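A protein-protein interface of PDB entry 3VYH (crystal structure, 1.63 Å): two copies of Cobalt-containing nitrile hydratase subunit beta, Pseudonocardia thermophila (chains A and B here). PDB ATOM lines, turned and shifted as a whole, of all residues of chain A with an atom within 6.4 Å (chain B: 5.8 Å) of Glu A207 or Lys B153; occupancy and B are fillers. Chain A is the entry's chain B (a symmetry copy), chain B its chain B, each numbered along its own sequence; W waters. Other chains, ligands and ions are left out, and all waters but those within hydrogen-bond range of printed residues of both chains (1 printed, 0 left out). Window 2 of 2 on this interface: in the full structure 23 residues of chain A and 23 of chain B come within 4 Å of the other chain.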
ATOM      1  N   ASP A  11      22.161  15.163   9.084  1.00  0.00           N
ATOM      2  CA  ASP A  11      23.544  15.317   9.533  1.00  0.00           C
ATOM      3  C   ASP A  11      24.045  14.085  10.314  1.00  0.00           C
ATOM      4  O   ASP A  11      23.275  13.359  10.880  1.00  0.00           O
ATOM      5  CB  ASP A  11      23.642  16.515  10.456  1.00  0.00           C
ATOM      6  CG  ASP A  11      23.381  17.842   9.744  1.00  0.00           C
ATOM      7  OD1 ASP A  11      23.820  17.979   8.574  1.00  0.00           O
ATOM      8  OD2 ASP A  11      22.775  18.792  10.381  1.00  0.00           O
ATOM      9  N   ALA A 200      18.760  27.031  -1.623  1.00  0.00           N
ATOM     10  CA  ALA A 200      19.372  26.380  -0.427  1.00  0.00           C
ATOM     11  C   ALA A 200      18.946  27.219   0.838  1.00  0.00           C
ATOM     12  O   ALA A 200      18.783  26.661   1.927  1.00  0.00           O
ATOM     13  CB  ALA A 200      20.909  26.433  -0.623  1.00  0.00           C
ATOM     14  N   GLN A 201      18.734  28.559   0.718  1.00  0.00           N
ATOM     15  CA  GLN A 201      18.239  29.366   1.884  1.00  0.00           C
ATOM     16  C   GLN A 201      16.845  28.969   2.332  1.00  0.00           C
ATOM     17  O   GLN A 201      16.525  28.946   3.488  1.00  0.00           O
ATOM     18  CB  GLN A 201      18.214  30.922   1.540  1.00  0.00           C
ATOM     19  CG  GLN A 201      19.467  31.454   0.835  1.00  0.00           C
ATOM     20  CD  GLN A 201      20.734  31.447   1.725  1.00  0.00           C
ATOM     21  OE1 GLN A 201      21.049  30.445   2.419  1.00  0.00           O
ATOM     22  NE2 GLN A 201      21.480  32.574   1.705  1.00  0.00           N
ATOM     23  N   TRP A 204      17.425  25.348   3.976  1.00  0.00           N
ATOM     24  CA  TRP A 204      18.331  25.184   5.155  1.00  0.00           C
ATOM     25  C   TRP A 204      18.414  26.418   6.058  1.00  0.00           C
ATOM     26  O   TRP A 204      19.071  26.401   7.076  1.00  0.00           O
ATOM     27  CB  TRP A 204      19.739  24.764   4.689  1.00  0.00           C
ATOM     28  CG  TRP A 204      19.669  23.623   3.673  1.00  0.00           C
ATOM     29  CD1 TRP A 204      20.149  23.664   2.373  1.00  0.00           C
ATOM     30  CD2 TRP A 204      19.097  22.297   3.853  1.00  0.00           C
ATOM     31  NE1 TRP A 204      19.911  22.468   1.741  1.00  0.00           N
ATOM     32  CE2 TRP A 204      19.261  21.631   2.610  1.00  0.00           C
ATOM     33  CE3 TRP A 204      18.458  21.628   4.926  1.00  0.00           C
ATOM     34  CZ2 TRP A 204      18.869  20.306   2.398  1.00  0.00           C
ATOM     35  CZ3 TRP A 204      17.997  20.280   4.686  1.00  0.00           C
ATOM     36  CH2 TRP A 204      18.176  19.696   3.396  1.00  0.00           C
ATOM     37  N   GLY A 205      17.722  27.479   5.669  1.00  0.00           N
ATOM     38  CA  GLY A 205      17.886  28.740   6.419  1.00  0.00           C
ATOM     39  C   GLY A 205      19.227  29.377   6.137  1.00  0.00           C
ATOM     40  O   GLY A 205      19.819  29.257   5.040  1.00  0.00           O
ATOM     41  N   PRO A 206      19.804  30.054   7.151  1.00  0.00           N
ATOM     42  CA  PRO A 206      21.100  30.760   6.890  1.00  0.00           C
ATOM     43  C   PRO A 206      22.306  29.803   6.772  1.00  0.00           C
ATOM     44  O   PRO A 206      23.291  30.185   6.177  1.00  0.00           O
ATOM     45  CB  PRO A 206      21.265  31.701   8.111  1.00  0.00           C
ATOM     46  CG  PRO A 206      20.191  31.241   9.178  1.00  0.00           C
ATOM     47  CD  PRO A 206      19.156  30.403   8.443  1.00  0.00           C
ATOM     48  N   GLU A 207      22.160  28.522   7.233  1.00  0.00           N
ATOM     49  CA  GLU A 207      23.203  27.480   7.053  1.00  0.00           C
ATOM     50  C   GLU A 207      23.273  26.919   5.616  1.00  0.00           C
ATOM     51  O   GLU A 207      24.193  26.165   5.273  1.00  0.00           O
ATOM     52  CB  GLU A 207      23.020  26.341   8.085  1.00  0.00           C
ATOM     53  CG  GLU A 207      23.363  26.740   9.593  1.00  0.00           C
ATOM     54  CD  GLU A 207      22.207  27.500  10.277  1.00  0.00           C
ATOM     55  OE1 GLU A 207      21.161  27.568   9.611  1.00  0.00           O
ATOM     56  OE2 GLU A 207      22.320  27.996  11.448  1.00  0.00           O
ATOM     57  N   GLY A 208      22.325  27.328   4.751  1.00  0.00           N
ATOM     58  CA  GLY A 208      22.372  26.902   3.339  1.00  0.00           C
ATOM     59  C   GLY A 208      23.504  27.572   2.572  1.00  0.00           C
ATOM     60  O   GLY A 208      23.914  28.692   2.901  1.00  0.00           O
ATOM     61  N   ASP A 209      24.036  26.850   1.584  1.00  0.00           N
ATOM     62  CA  ASP A 209      24.929  27.498   0.608  1.00  0.00           C
ATOM     63  C   ASP A 209      24.324  28.784  -0.016  1.00  0.00           C
ATOM     64  O   ASP A 209      23.187  28.854  -0.529  1.00  0.00           O
ATOM     65  CB  ASP A 209      25.308  26.438  -0.426  1.00  0.00           C
ATOM     66  CG  ASP A 209      26.497  26.850  -1.325  1.00  0.00           C
ATOM     67  OD1 ASP A 209      26.327  27.782  -2.091  1.00  0.00           O
ATOM     68  OD2 ASP A 209      27.560  26.232  -1.204  1.00  0.00           O
ATOM     69  N   MET B   1      22.014  20.055  15.119  1.00  0.00           N
ATOM     70  CA  MET B   1      22.313  19.252  13.878  1.00  0.00           C
ATOM     71  C   MET B   1      21.043  18.465  13.544  1.00  0.00           C
ATOM     72  O   MET B   1      20.208  18.102  14.426  1.00  0.00           O
ATOM     73  CB  MET B   1      23.553  18.343  14.191  1.00  0.00           C
ATOM     74  CG  MET B   1      23.252  17.201  15.209  1.00  0.00           C
ATOM     75  SD  MET B   1      24.705  16.132  15.435  1.00  0.00           S
ATOM     76  CE  MET B   1      24.562  15.105  13.953  1.00  0.00           C
ATOM     77  N   PHE B  53      25.124  17.015  23.078  1.00  0.00           N
ATOM     78  CA  PHE B  53      25.633  17.118  21.709  1.00  0.00           C
ATOM     79  C   PHE B  53      26.546  15.922  21.367  1.00  0.00           C
ATOM     80  O   PHE B  53      26.581  15.416  20.230  1.00  0.00           O
ATOM     81  CB  PHE B  53      26.354  18.464  21.519  1.00  0.00           C
ATOM     82  CG  PHE B  53      26.819  18.728  20.120  1.00  0.00           C
ATOM     83  CD1 PHE B  53      26.036  18.344  19.006  1.00  0.00           C
ATOM     84  CD2 PHE B  53      28.019  19.403  19.893  1.00  0.00           C
ATOM     85  CE1 PHE B  53      26.471  18.566  17.694  1.00  0.00           C
ATOM     86  CE2 PHE B  53      28.480  19.642  18.583  1.00  0.00           C
ATOM     87  CZ  PHE B  53      27.743  19.217  17.470  1.00  0.00           C
ATOM     88  N   THR B 149      13.438  28.079  10.473  1.00  0.00           N
ATOM     89  CA  THR B 149      13.926  27.001   9.606  1.00  0.00           C
ATOM     90  C   THR B 149      15.463  26.999   9.540  1.00  0.00           C
ATOM     91  O   THR B 149      16.058  26.309   8.638  1.00  0.00           O
ATOM     92  CB  THR B 149      13.302  27.109   8.235  1.00  0.00           C
ATOM     93  OG1 THR B 149      13.582  28.438   7.750  1.00  0.00           O
ATOM     94  CG2 THR B 149      11.753  26.861   8.316  1.00  0.00           C
ATOM     95  N   ALA B 150      16.151  27.649  10.494  1.00  0.00           N
ATOM     96  CA  ALA B 150      17.580  27.519  10.520  1.00  0.00           C
ATOM     97  C   ALA B 150      17.942  26.080  10.843  1.00  0.00           C
ATOM     98  O   ALA B 150      17.183  25.373  11.502  1.00  0.00           O
ATOM     99  CB  ALA B 150      18.246  28.488  11.572  1.00  0.00           C
ATOM    100  N   SER B 151      19.155  25.725  10.443  1.00  0.00           N
ATOM    101  CA  SER B 151      19.544  24.237  10.577  1.00  0.00           C
ATOM    102  C   SER B 151      21.000  24.171  11.044  1.00  0.00           C
ATOM    103  O   SER B 151      21.936  23.762  10.300  1.00  0.00           O
ATOM    104  CB  SER B 151      19.245  23.500   9.245  1.00  0.00           C
ATOM    105  OG  SER B 151      19.947  24.141   8.146  1.00  0.00           O
ATOM    106  N   PRO B 152      21.235  24.662  12.253  1.00  0.00           N
ATOM    107  CA  PRO B 152      22.665  24.665  12.669  1.00  0.00           C
ATOM    108  C   PRO B 152      23.319  23.272  12.604  1.00  0.00           C
ATOM    109  O   PRO B 152      22.676  22.210  12.864  1.00  0.00           O
ATOM    110  CB  PRO B 152      22.621  25.178  14.113  1.00  0.00           C
ATOM    111  CG  PRO B 152      21.201  25.078  14.546  1.00  0.00           C
ATOM    112  CD  PRO B 152      20.311  25.084  13.308  1.00  0.00           C
ATOM    113  N   LYS B 153      24.596  23.300  12.282  1.00  0.00           N
ATOM    114  CA  LYS B 153      25.296  22.036  12.225  1.00  0.00           C
ATOM    115  C   LYS B 153      25.820  21.555  13.570  1.00  0.00           C
ATOM    116  O   LYS B 153      26.221  20.345  13.680  1.00  0.00           O
ATOM    117  CB  LYS B 153      26.477  22.157  11.236  1.00  0.00           C
ATOM    118  CG  LYS B 153      25.885  22.321   9.765  1.00  0.00           C
ATOM    119  CD  LYS B 153      26.801  23.042   8.732  1.00  0.00           C
ATOM    120  CE  LYS B 153      25.992  23.197   7.418  1.00  0.00           C
ATOM    121  NZ  LYS B 153      26.989  23.518   6.297  1.00  0.00           N
ATOM    122  N   GLY B 154      25.944  22.467  14.553  1.00  0.00           N
ATOM    123  CA  GLY B 154      26.308  22.128  15.960  1.00  0.00           C
ATOM    124  C   GLY B 154      25.047  21.811  16.756  1.00  0.00           C
ATOM    125  O   GLY B 154      23.958  21.638  16.159  1.00  0.00           O
ATOM    126  N   HIS B 155      25.188  21.841  18.070  1.00  0.00           N
ATOM    127  CA  HIS B 155      24.045  21.537  18.937  1.00  0.00           C
ATOM    128  C   HIS B 155      22.951  22.634  18.856  1.00  0.00           C
ATOM    129  O   HIS B 155      23.275  23.827  18.783  1.00  0.00           O
ATOM    130  CB  HIS B 155      24.539  21.435  20.381  1.00  0.00           C
ATOM    131  CG  HIS B 155      23.462  21.061  21.358  1.00  0.00           C
ATOM    132  ND1 HIS B 155      22.833  19.840  21.364  1.00  0.00           N
ATOM    133  CD2 HIS B 155      22.869  21.801  22.332  1.00  0.00           C
ATOM    134  CE1 HIS B 155      21.934  19.827  22.329  1.00  0.00           C
ATOM    135  NE2 HIS B 155      21.955  20.976  22.959  1.00  0.00           N
HETATM  136  O   HOH W   1      25.791  24.010   4.124  1.00  0.00           O
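The backbone carbonyl oxygen (O) of Gly B154 is in hydrogen-bond range of the backbone NH (N) of Met B1 (2.7 Å). O of Pro B152 sits close to N of Met B1, 3.2 Å away. The backbone carbonyl oxygen of Gly A205 sits close to the side-chain amide oxygen of Gln A201.
Hydrophobic or aromatic side chains of chain A that line the printed part of chain B: Trp A204 and Pro A206. Of the 9 printed residues of chain B, 6 touch a printed residue of chain A. Among the printed residues, no Asp or Glu carboxylate lies within 4 Å of a Lys or Arg side-chain nitrogen of the other chain.
The side-chain hydroxyl of Ser B151 lies within hydrogen-bond range of the backbone carbonyl oxygen of Trp A204 (2.6 Å). N of Ser B151 lies within hydrogen-bond range of OE1 of Glu A207, at 2.8 Å. The backbone carbonyl oxygen (O) of Trp A204 lies close to the backbone carbonyl oxygen (O) of Thr B149, 3.4 Å away.
Printed residues of chain B within 4 Å of Glu A207: Ala B150, Ser B151, Pro B152 and Lys B153. Printed residues of chain A within 4 Å of Lys B153: Glu A207 (3.98 Å). Of the printed residues of chain A, Met B1 touches Asp A11 (3.6 Å). Printed residues of chain A within 4 Å of Thr B149: Trp A204 and Gly A205. Printed residues of chain B within 4 Å of Pro A206: Ala B150 (3.8 Å). Phe B53 touches none of the printed residues of chain A. Gly B154 touches none of the printed residues of chain A. The nearest printed residue of chain A that does not touch Lys B153 is Asp A11 (4.5 Å).
Asp A11 touches Met B1. O of Trp A204 touches CA of Ala B150, at 3.9 Å. O of Thr B149 touches N of Gly A205, at 3.6 Å. Pro A206 touches Ala B150. Ala B150 touches Glu A207. Glu A207 touches Pro B152. O of Glu A207 touches NZ of Lys B153, at 3.98 Å.
Water W1 bridges NZ of Lys B153 and O of Glu A207.
No position is printed for both chains. Of the 10 pairs that touch across the chains among the printed residues, none has its exchanged pair printed and touching as well.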
